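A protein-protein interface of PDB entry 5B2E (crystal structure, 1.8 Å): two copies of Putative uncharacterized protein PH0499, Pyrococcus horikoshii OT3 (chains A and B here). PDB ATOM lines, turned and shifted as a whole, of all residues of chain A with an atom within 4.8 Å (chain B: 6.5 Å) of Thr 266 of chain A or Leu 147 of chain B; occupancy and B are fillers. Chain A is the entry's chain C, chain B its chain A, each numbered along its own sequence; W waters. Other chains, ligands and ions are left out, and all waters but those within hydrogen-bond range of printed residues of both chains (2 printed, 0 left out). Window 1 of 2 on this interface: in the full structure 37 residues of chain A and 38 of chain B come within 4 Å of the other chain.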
ATOM      1  N   TRP A 146      34.977  -9.489 -34.582  1.00  0.00           N
ATOM      2  CA  TRP A 146      34.547 -10.592 -35.405  1.00  0.00           C
ATOM      3  C   TRP A 146      34.472 -10.267 -36.893  1.00  0.00           C
ATOM      4  O   TRP A 146      33.913 -11.030 -37.661  1.00  0.00           O
ATOM      5  CB  TRP A 146      33.231 -11.154 -34.882  1.00  0.00           C
ATOM      6  CG  TRP A 146      33.390 -11.736 -33.488  1.00  0.00           C
ATOM      7  CD1 TRP A 146      33.810 -13.014 -33.145  1.00  0.00           C
ATOM      8  CD2 TRP A 146      33.138 -11.048 -32.257  1.00  0.00           C
ATOM      9  NE1 TRP A 146      33.875 -13.121 -31.765  1.00  0.00           N
ATOM     10  CE2 TRP A 146      33.442 -11.945 -31.203  1.00  0.00           C
ATOM     11  CE3 TRP A 146      32.661  -9.764 -31.950  1.00  0.00           C
ATOM     12  CZ2 TRP A 146      33.292 -11.595 -29.856  1.00  0.00           C
ATOM     13  CZ3 TRP A 146      32.507  -9.408 -30.604  1.00  0.00           C
ATOM     14  CH2 TRP A 146      32.812 -10.314 -29.578  1.00  0.00           C
ATOM     15  N   LEU A 261      23.540  -9.103 -22.683  1.00  0.00           N
ATOM     16  CA  LEU A 261      23.550 -10.604 -22.481  1.00  0.00           C
ATOM     17  C   LEU A 261      23.998 -11.379 -23.744  1.00  0.00           C
ATOM     18  O   LEU A 261      24.549 -12.541 -23.633  1.00  0.00           O
ATOM     19  CB  LEU A 261      22.156 -11.169 -22.121  1.00  0.00           C
ATOM     20  CG  LEU A 261      21.605 -10.822 -20.697  1.00  0.00           C
ATOM     21  CD1 LEU A 261      20.429 -11.756 -20.326  1.00  0.00           C
ATOM     22  CD2 LEU A 261      22.699 -10.844 -19.612  1.00  0.00           C
ATOM     23  N   PHE A 262      23.767 -10.760 -24.901  1.00  0.00           N
ATOM     24  CA  PHE A 262      24.029 -11.435 -26.187  1.00  0.00           C
ATOM     25  C   PHE A 262      25.512 -11.542 -26.500  1.00  0.00           C
ATOM     26  O   PHE A 262      25.914 -12.267 -27.449  1.00  0.00           O
ATOM     27  CB  PHE A 262      23.353 -10.694 -27.329  1.00  0.00           C
ATOM     28  CG  PHE A 262      21.905 -11.031 -27.517  1.00  0.00           C
ATOM     29  CD1 PHE A 262      21.078 -11.385 -26.448  1.00  0.00           C
ATOM     30  CD2 PHE A 262      21.334 -10.937 -28.799  1.00  0.00           C
ATOM     31  CE1 PHE A 262      19.719 -11.668 -26.645  1.00  0.00           C
ATOM     32  CE2 PHE A 262      19.987 -11.201 -28.989  1.00  0.00           C
ATOM     33  CZ  PHE A 262      19.161 -11.552 -27.908  1.00  0.00           C
ATOM     34  N   HIS A 264      27.470 -13.062 -24.777  1.00  0.00           N
ATOM     35  CA  HIS A 264      27.955 -14.228 -23.980  1.00  0.00           C
ATOM     36  C   HIS A 264      26.947 -15.349 -24.108  1.00  0.00           C
ATOM     37  O   HIS A 264      25.725 -15.161 -23.933  1.00  0.00           O
ATOM     38  CB  HIS A 264      28.073 -13.850 -22.459  1.00  0.00           C
ATOM     39  CG  HIS A 264      28.886 -14.834 -21.645  1.00  0.00           C
ATOM     40  ND1 HIS A 264      30.089 -15.337 -22.067  1.00  0.00           N
ATOM     41  CD2 HIS A 264      28.675 -15.362 -20.405  1.00  0.00           C
ATOM     42  CE1 HIS A 264      30.594 -16.144 -21.155  1.00  0.00           C
ATOM     43  NE2 HIS A 264      29.741 -16.194 -20.145  1.00  0.00           N
ATOM     44  N   ILE A 265      27.499 -16.539 -24.429  1.00  0.00           N
ATOM     45  CA  ILE A 265      26.755 -17.827 -24.527  1.00  0.00           C
ATOM     46  C   ILE A 265      25.496 -17.817 -25.415  1.00  0.00           C
ATOM     47  O   ILE A 265      24.667 -18.696 -25.314  1.00  0.00           O
ATOM     48  CB  ILE A 265      26.495 -18.483 -23.128  1.00  0.00           C
ATOM     49  CG1 ILE A 265      25.385 -17.750 -22.305  1.00  0.00           C
ATOM     50  CG2 ILE A 265      27.862 -18.620 -22.419  1.00  0.00           C
ATOM     51  CD1 ILE A 265      24.943 -18.572 -20.987  1.00  0.00           C
ATOM     52  N   THR A 266      25.409 -16.900 -26.354  1.00  0.00           N
ATOM     53  CA  THR A 266      24.112 -16.728 -27.000  1.00  0.00           C
ATOM     54  C   THR A 266      24.200 -17.360 -28.400  1.00  0.00           C
ATOM     55  O   THR A 266      24.952 -16.867 -29.238  1.00  0.00           O
ATOM     56  CB  THR A 266      23.750 -15.199 -27.125  1.00  0.00           C
ATOM     57  OG1 THR A 266      23.557 -14.727 -25.790  1.00  0.00           O
ATOM     58  CG2 THR A 266      22.439 -14.987 -27.954  1.00  0.00           C
ATOM     59  N   PRO A 267      23.299 -18.273 -28.683  1.00  0.00           N
ATOM     60  CA  PRO A 267      23.434 -18.980 -30.014  1.00  0.00           C
ATOM     61  C   PRO A 267      22.633 -18.403 -31.171  1.00  0.00           C
ATOM     62  O   PRO A 267      22.722 -18.997 -32.268  1.00  0.00           O
ATOM     63  CB  PRO A 267      22.931 -20.382 -29.719  1.00  0.00           C
ATOM     64  CG  PRO A 267      21.875 -20.134 -28.612  1.00  0.00           C
ATOM     65  CD  PRO A 267      22.451 -19.043 -27.726  1.00  0.00           C
ATOM     66  N   PHE A 268      21.931 -17.255 -30.953  1.00  0.00           N
ATOM     67  CA  PHE A 268      21.026 -16.665 -31.963  1.00  0.00           C
ATOM     68  C   PHE A 268      21.331 -15.143 -32.142  1.00  0.00           C
ATOM     69  O   PHE A 268      20.433 -14.373 -32.445  1.00  0.00           O
ATOM     70  CB  PHE A 268      19.526 -16.992 -31.618  1.00  0.00           C
ATOM     71  CG  PHE A 268      19.149 -16.804 -30.120  1.00  0.00           C
ATOM     72  CD1 PHE A 268      18.695 -17.849 -29.333  1.00  0.00           C
ATOM     73  CD2 PHE A 268      19.280 -15.569 -29.515  1.00  0.00           C
ATOM     74  CE1 PHE A 268      18.340 -17.673 -27.935  1.00  0.00           C
ATOM     75  CE2 PHE A 268      18.977 -15.374 -28.132  1.00  0.00           C
ATOM     76  CZ  PHE A 268      18.447 -16.425 -27.333  1.00  0.00           C
ATOM     77  N   THR A 269      22.591 -14.753 -31.982  1.00  0.00           N
ATOM     78  CA  THR A 269      22.956 -13.326 -32.114  1.00  0.00           C
ATOM     79  C   THR A 269      22.688 -12.854 -33.571  1.00  0.00           C
ATOM     80  O   THR A 269      22.569 -11.647 -33.811  1.00  0.00           O
ATOM     81  CB  THR A 269      24.429 -13.070 -31.832  1.00  0.00           C
ATOM     82  OG1 THR A 269      25.238 -13.869 -32.724  1.00  0.00           O
ATOM     83  CG2 THR A 269      24.814 -13.355 -30.327  1.00  0.00           C
ATOM     84  N   ASP B 144      31.945 -24.382 -27.422  1.00  0.00           N
ATOM     85  CA  ASP B 144      32.323 -24.208 -28.820  1.00  0.00           C
ATOM     86  C   ASP B 144      33.098 -22.930 -28.910  1.00  0.00           C
ATOM     87  O   ASP B 144      32.539 -21.864 -28.730  1.00  0.00           O
ATOM     88  CB  ASP B 144      31.053 -24.149 -29.657  1.00  0.00           C
ATOM     89  CG  ASP B 144      31.332 -24.043 -31.163  1.00  0.00           C
ATOM     90  OD1 ASP B 144      30.430 -24.388 -31.939  1.00  0.00           O
ATOM     91  OD2 ASP B 144      32.465 -23.746 -31.519  1.00  0.00           O
ATOM     92  N   PRO B 145      34.386 -22.996 -29.174  1.00  0.00           N
ATOM     93  CA  PRO B 145      35.093 -21.677 -29.211  1.00  0.00           C
ATOM     94  C   PRO B 145      34.798 -20.879 -30.424  1.00  0.00           C
ATOM     95  O   PRO B 145      35.284 -19.721 -30.570  1.00  0.00           O
ATOM     96  CB  PRO B 145      36.578 -22.058 -29.239  1.00  0.00           C
ATOM     97  CG  PRO B 145      36.594 -23.471 -29.863  1.00  0.00           C
ATOM     98  CD  PRO B 145      35.299 -24.152 -29.427  1.00  0.00           C
ATOM     99  N   TRP B 146      34.014 -21.440 -31.330  1.00  0.00           N
ATOM    100  CA  TRP B 146      33.692 -20.681 -32.562  1.00  0.00           C
ATOM    101  C   TRP B 146      32.363 -19.924 -32.474  1.00  0.00           C
ATOM    102  O   TRP B 146      31.905 -19.401 -33.481  1.00  0.00           O
ATOM    103  CB  TRP B 146      33.745 -21.564 -33.875  1.00  0.00           C
ATOM    104  CG  TRP B 146      35.187 -21.979 -34.189  1.00  0.00           C
ATOM    105  CD1 TRP B 146      36.114 -21.260 -34.882  1.00  0.00           C
ATOM    106  CD2 TRP B 146      35.843 -23.146 -33.734  1.00  0.00           C
ATOM    107  NE1 TRP B 146      37.303 -21.916 -34.895  1.00  0.00           N
ATOM    108  CE2 TRP B 146      37.161 -23.090 -34.208  1.00  0.00           C
ATOM    109  CE3 TRP B 146      35.410 -24.283 -33.057  1.00  0.00           C
ATOM    110  CZ2 TRP B 146      38.080 -24.090 -33.975  1.00  0.00           C
ATOM    111  CZ3 TRP B 146      36.305 -25.288 -32.823  1.00  0.00           C
ATOM    112  CH2 TRP B 146      37.634 -25.186 -33.274  1.00  0.00           C
ATOM    113  N   LEU B 147      31.769 -19.826 -31.290  1.00  0.00           N
ATOM    114  CA  LEU B 147      30.502 -19.147 -31.106  1.00  0.00           C
ATOM    115  C   LEU B 147      30.646 -17.657 -31.447  1.00  0.00           C
ATOM    116  O   LEU B 147      31.532 -17.000 -30.908  1.00  0.00           O
ATOM    117  CB  LEU B 147      30.172 -19.201 -29.640  1.00  0.00           C
ATOM    118  CG  LEU B 147      28.757 -19.127 -29.135  1.00  0.00           C
ATOM    119  CD1 LEU B 147      28.561 -18.550 -27.733  1.00  0.00           C
ATOM    120  CD2 LEU B 147      27.393 -19.405 -29.817  1.00  0.00           C
ATOM    121  N   PRO B 148      29.811 -17.151 -32.351  1.00  0.00           N
ATOM    122  CA  PRO B 148      30.064 -15.773 -32.730  1.00  0.00           C
ATOM    123  C   PRO B 148      29.700 -14.830 -31.570  1.00  0.00           C
ATOM    124  O   PRO B 148      28.799 -15.145 -30.746  1.00  0.00           O
ATOM    125  CB  PRO B 148      29.087 -15.567 -33.926  1.00  0.00           C
ATOM    126  CG  PRO B 148      29.138 -16.945 -34.663  1.00  0.00           C
ATOM    127  CD  PRO B 148      28.921 -17.838 -33.331  1.00  0.00           C
ATOM    128  N   TYR B 149      30.434 -13.725 -31.493  1.00  0.00           N
ATOM    129  CA  TYR B 149      30.094 -12.711 -30.504  1.00  0.00           C
ATOM    130  C   TYR B 149      30.304 -13.180 -29.037  1.00  0.00           C
ATOM    131  O   TYR B 149      30.004 -12.435 -28.072  1.00  0.00           O
ATOM    132  CB  TYR B 149      28.683 -12.049 -30.801  1.00  0.00           C
ATOM    133  CG  TYR B 149      28.812 -11.239 -32.049  1.00  0.00           C
ATOM    134  CD1 TYR B 149      29.322  -9.962 -31.995  1.00  0.00           C
ATOM    135  CD2 TYR B 149      28.512 -11.789 -33.294  1.00  0.00           C
ATOM    136  CE1 TYR B 149      29.531  -9.222 -33.166  1.00  0.00           C
ATOM    137  CE2 TYR B 149      28.730 -11.023 -34.500  1.00  0.00           C
ATOM    138  CZ  TYR B 149      29.257  -9.780 -34.404  1.00  0.00           C
ATOM    139  OH  TYR B 149      29.533  -8.989 -35.610  1.00  0.00           O
ATOM    140  N   GLU B 150      30.985 -14.309 -28.873  1.00  0.00           N
ATOM    141  CA  GLU B 150      31.335 -14.779 -27.541  1.00  0.00           C
ATOM    142  C   GLU B 150      32.499 -13.890 -27.054  1.00  0.00           C
ATOM    143  O   GLU B 150      33.605 -13.985 -27.531  1.00  0.00           O
ATOM    144  CB  GLU B 150      31.722 -16.279 -27.500  1.00  0.00           C
ATOM    145  CG  GLU B 150      32.360 -16.636 -26.206  1.00  0.00           C
ATOM    146  CD  GLU B 150      31.352 -16.401 -24.995  1.00  0.00           C
ATOM    147  OE1 GLU B 150      30.285 -17.072 -24.920  1.00  0.00           O
ATOM    148  OE2 GLU B 150      31.559 -15.386 -24.201  1.00  0.00           O
ATOM    149  N   SER B 151      32.215 -12.964 -26.119  1.00  0.00           N
ATOM    150  CA  SER B 151      33.187 -11.955 -25.760  1.00  0.00           C
ATOM    151  C   SER B 151      33.984 -12.271 -24.468  1.00  0.00           C
ATOM    152  O   SER B 151      34.857 -11.538 -24.039  1.00  0.00           O
ATOM    153  CB  SER B 151      32.473 -10.612 -25.633  1.00  0.00           C
ATOM    154  OG  SER B 151      31.773 -10.648 -24.388  1.00  0.00           O
ATOM    155  N   ARG B 156      36.274 -18.731 -24.895  1.00  0.00           N
ATOM    156  CA  ARG B 156      36.890 -19.045 -26.162  1.00  0.00           C
ATOM    157  C   ARG B 156      38.141 -19.901 -25.895  1.00  0.00           C
ATOM    158  O   ARG B 156      38.412 -20.952 -26.575  1.00  0.00           O
ATOM    159  CB  ARG B 156      37.271 -17.736 -26.858  1.00  0.00           C
ATOM    160  CG  ARG B 156      36.041 -16.878 -27.163  1.00  0.00           C
ATOM    161  CD  ARG B 156      36.451 -15.737 -28.118  1.00  0.00           C
ATOM    162  NE  ARG B 156      37.657 -15.005 -27.648  1.00  0.00           N
ATOM    163  CZ  ARG B 156      37.629 -13.808 -27.081  1.00  0.00           C
ATOM    164  NH1 ARG B 156      36.464 -13.160 -26.925  1.00  0.00           N
ATOM    165  NH2 ARG B 156      38.765 -13.232 -26.689  1.00  0.00           N
ATOM    166  N   TYR B 196      27.125 -24.691 -25.754  1.00  0.00           N
ATOM    167  CA  TYR B 196      27.117 -23.248 -26.015  1.00  0.00           C
ATOM    168  C   TYR B 196      27.470 -23.032 -27.483  1.00  0.00           C
ATOM    169  O   TYR B 196      28.425 -22.319 -27.838  1.00  0.00           O
ATOM    170  CB  TYR B 196      28.142 -22.534 -25.187  1.00  0.00           C
ATOM    171  CG  TYR B 196      27.832 -22.395 -23.675  1.00  0.00           C
ATOM    172  CD1 TYR B 196      26.542 -22.305 -23.225  1.00  0.00           C
ATOM    173  CD2 TYR B 196      28.930 -22.264 -22.753  1.00  0.00           C
ATOM    174  CE1 TYR B 196      26.302 -22.027 -21.873  1.00  0.00           C
ATOM    175  CE2 TYR B 196      28.689 -22.032 -21.373  1.00  0.00           C
ATOM    176  CZ  TYR B 196      27.382 -21.886 -20.965  1.00  0.00           C
ATOM    177  OH  TYR B 196      27.222 -21.603 -19.605  1.00  0.00           O
ATOM    178  N   THR B 197      26.702 -23.696 -28.341  1.00  0.00           N
ATOM    179  CA  THR B 197      27.036 -23.597 -29.780  1.00  0.00           C
ATOM    180  C   THR B 197      25.920 -22.993 -30.608  1.00  0.00           C
ATOM    181  O   THR B 197      24.752 -23.157 -30.310  1.00  0.00           O
ATOM    182  CB  THR B 197      27.381 -25.041 -30.354  1.00  0.00           C
ATOM    183  OG1 THR B 197      27.714 -24.889 -31.733  1.00  0.00           O
ATOM    184  CG2 THR B 197      26.201 -26.010 -30.159  1.00  0.00           C
ATOM    185  N   HIS B 198      26.320 -22.312 -31.703  1.00  0.00           N
ATOM    186  CA  HIS B 198      25.398 -21.706 -32.612  1.00  0.00           C
ATOM    187  C   HIS B 198      25.106 -22.666 -33.763  1.00  0.00           C
ATOM    188  O   HIS B 198      24.176 -22.415 -34.524  1.00  0.00           O
ATOM    189  CB  HIS B 198      26.085 -20.499 -33.256  1.00  0.00           C
ATOM    190  CG  HIS B 198      27.490 -20.777 -33.740  1.00  0.00           C
ATOM    191  ND1 HIS B 198      27.929 -20.403 -35.012  1.00  0.00           N
ATOM    192  CD2 HIS B 198      28.554 -21.411 -33.145  1.00  0.00           C
ATOM    193  CE1 HIS B 198      29.187 -20.785 -35.170  1.00  0.00           C
ATOM    194  NE2 HIS B 198      29.583 -21.406 -34.064  1.00  0.00           N
ATOM    195  N   LYS B 199      25.884 -23.745 -33.853  1.00  0.00           N
ATOM    196  CA  LYS B 199      25.660 -24.763 -34.935  1.00  0.00           C
ATOM    197  C   LYS B 199      25.437 -26.177 -34.389  1.00  0.00           C
ATOM    198  O   LYS B 199      26.188 -27.124 -34.705  1.00  0.00           O
ATOM    199  CB  LYS B 199      26.815 -24.753 -35.915  1.00  0.00           C
ATOM    200  CG  LYS B 199      26.857 -23.477 -36.775  1.00  0.00           C
ATOM    201  CD  LYS B 199      25.750 -23.480 -37.826  1.00  0.00           C
ATOM    202  CE  LYS B 199      25.529 -22.084 -38.475  1.00  0.00           C
ATOM    203  NZ  LYS B 199      24.387 -22.199 -39.479  1.00  0.00           N
ATOM    204  N   PHE B 235      16.167 -15.571 -20.347  1.00  0.00           N
ATOM    205  CA  PHE B 235      17.265 -15.735 -21.305  1.00  0.00           C
ATOM    206  C   PHE B 235      17.544 -17.250 -21.390  1.00  0.00           C
ATOM    207  O   PHE B 235      17.639 -17.805 -22.489  1.00  0.00           O
ATOM    208  CB  PHE B 235      18.482 -15.126 -20.704  1.00  0.00           C
ATOM    209  CG  PHE B 235      19.749 -15.251 -21.506  1.00  0.00           C
ATOM    210  CD1 PHE B 235      19.807 -14.696 -22.819  1.00  0.00           C
ATOM    211  CD2 PHE B 235      20.938 -15.663 -20.897  1.00  0.00           C
ATOM    212  CE1 PHE B 235      21.011 -14.708 -23.574  1.00  0.00           C
ATOM    213  CE2 PHE B 235      22.163 -15.687 -21.656  1.00  0.00           C
ATOM    214  CZ  PHE B 235      22.167 -15.169 -23.028  1.00  0.00           C
ATOM    215  N   ILE B 239      16.982 -19.648 -24.688  1.00  0.00           N
ATOM    216  CA  ILE B 239      18.030 -20.491 -25.299  1.00  0.00           C
ATOM    217  C   ILE B 239      17.589 -21.943 -25.343  1.00  0.00           C
ATOM    218  O   ILE B 239      17.810 -22.635 -26.382  1.00  0.00           O
ATOM    219  CB  ILE B 239      19.355 -20.374 -24.517  1.00  0.00           C
ATOM    220  CG1 ILE B 239      19.909 -18.923 -24.559  1.00  0.00           C
ATOM    221  CG2 ILE B 239      20.408 -21.516 -24.919  1.00  0.00           C
ATOM    222  CD1 ILE B 239      21.105 -18.758 -23.751  1.00  0.00           C
ATOM    223  N   TYR B 243      17.124 -24.397 -28.922  1.00  0.00           N
ATOM    224  CA  TYR B 243      17.617 -25.776 -29.141  1.00  0.00           C
ATOM    225  C   TYR B 243      16.453 -26.791 -29.272  1.00  0.00           C
ATOM    226  O   TYR B 243      16.461 -27.642 -30.200  1.00  0.00           O
ATOM    227  CB  TYR B 243      18.666 -26.217 -28.081  1.00  0.00           C
ATOM    228  CG  TYR B 243      19.958 -25.456 -28.077  1.00  0.00           C
ATOM    229  CD1 TYR B 243      20.711 -25.283 -29.252  1.00  0.00           C
ATOM    230  CD2 TYR B 243      20.409 -24.793 -26.890  1.00  0.00           C
ATOM    231  CE1 TYR B 243      21.931 -24.625 -29.237  1.00  0.00           C
ATOM    232  CE2 TYR B 243      21.635 -24.095 -26.866  1.00  0.00           C
ATOM    233  CZ  TYR B 243      22.377 -24.014 -28.011  1.00  0.00           C
ATOM    234  OH  TYR B 243      23.531 -23.345 -27.942  1.00  0.00           O
HETATM  235  O   HOH W   1      24.173 -21.467 -25.713  1.00  0.00           O
HETATM  236  O   HOH W   2      26.358 -16.406 -31.492  1.00  0.00           O
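The backbone carbonyl oxygen (O) of Leu 261 of chain A lies within hydrogen-bond range of the side-chain hydroxyl (OG1) of Thr 266 of chain A, at 3.2 Å.
O of Glu 150 of chain B is in hydrogen-bond range of NH1 of Arg 156 of chain B.
O of His 264 of chain A lies within hydrogen-bond range of OG1 of Thr 266 of chain A (2.9 Å).
OG1 of Thr 197 of chain B is in hydrogen-bond range of N of Lys 199 of chain B (3.0 Å).
O of Thr 197 of chain B is in hydrogen-bond range of OH of Tyr 243 of chain B.
OD1 of Asp 144 of chain B is in hydrogen-bond range of OG1 of Thr 197 of chain B (2.8 Å).
Water W2 lies within hydrogen-bond range of O of Thr 266 of chain A (2.7 Å), O of Pro 148 of chain B (2.8 Å) and OG1 of Thr 269 of chain A (3.0 Å).
Water W1 bridges the backbone carbonyl oxygen of Ile 265 of chain A and the side-chain hydroxyl of Tyr 243 of chain B.
Of the printed residues of chain B, Leu 261 of chain A touches Phe 235 (3.6 Å).
Of the printed residues of chain B, Pro 267 of chain A touches Leu 147 (3.99 Å), Thr 197 (3.4 Å), His 198 (3.8 Å) and Tyr 243 (3.5 Å).
Printed residues of chain B within 4 Å of Phe 268 of chain A: Ile 239.
Printed residues of chain B within 4 Å of Thr 269 of chain A: Tyr 149.
Of the printed residues of chain A, Tyr 243 of chain B touches Pro 267 (3.5 Å).
The nearest residue of chain B that does not touch Thr 266 of chain A is Pro 148 of chain B (4.5 Å).
The nearest printed residue of chain A that does not touch Leu 147 of chain B is Trp 146 of chain A (4.6 Å).
Of the 9 printed residues of chain A, 8 touch a printed residue of chain B.
Hydrophobic or aromatic side chains of chain A that line the printed part of chain B: Trp 146, Leu 261, His 264, Ile 265, Pro 267 and Phe 268.
Printed residues of chain B that touch a printed residue of chain A: Leu 147, Tyr 149, Glu 150, Ser 151, Tyr 196, Thr 197, His 198, Phe 235, Ile 239 and Tyr 243.
Hydrophobic or aromatic side chains of chain B within 4 Å of the printed part of chain A: Leu 147, Tyr 149, Tyr 196, His 198, Phe 235, Ile 239 and Tyr 243.
Among the printed residues, 19 pairs touch across the chains.
Among the printed residues, no Asp or Glu carboxylate lies within 4 Å of a Lys or Arg side-chain nitrogen of the other chain.
1 position is printed for both chains.
Of the 19 pairs that touch across the chains among the printed residues, none has its exchanged pair printed and touching as well.
CZ2 of Trp 146 of chain A touches O of Glu 150 of chain B, 3.3 Å away.
Trp 146 of chain A touches Ser 151 of chain B (CH2 to CB, 3.97 Å).
CZ of Phe 235 of chain B touches O of Leu 261 of chain A (3.6 Å).
Phe 235 of chain B touches His 264 of chain A (CZ to O, 3.7 Å).
CZ of Tyr 196 of chain B touches CG2 of Ile 265 of chain A, 3.6 Å away.
CG1 of Ile 265 of chain A touches CE2 of Phe 235 of chain B (3.9 Å).
O of Ile 265 of chain A touches CD1 of Ile 239 of chain B, 3.9 Å away.
Leu 147 of chain B touches Thr 266 of chain A (CD2 to O, 3.6 Å).
Thr 197 of chain B touches Pro 267 of chain A (O to CB, 3.4 Å).
Tyr 149 of chain B touches Thr 269 of chain A (CD2 to OG1, 3.9 Å).
The side-chain carboxylate (OE1) of Glu 150 of chain B is in hydrogen-bond range of the backbone NH (N) of Ile 265 of chain A (2.9 Å).
A ring nitrogen (ND1) of His 264 of chain A is in hydrogen-bond range of the side-chain carboxylate (OE2) of Glu 150 of chain B (2.6 Å).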
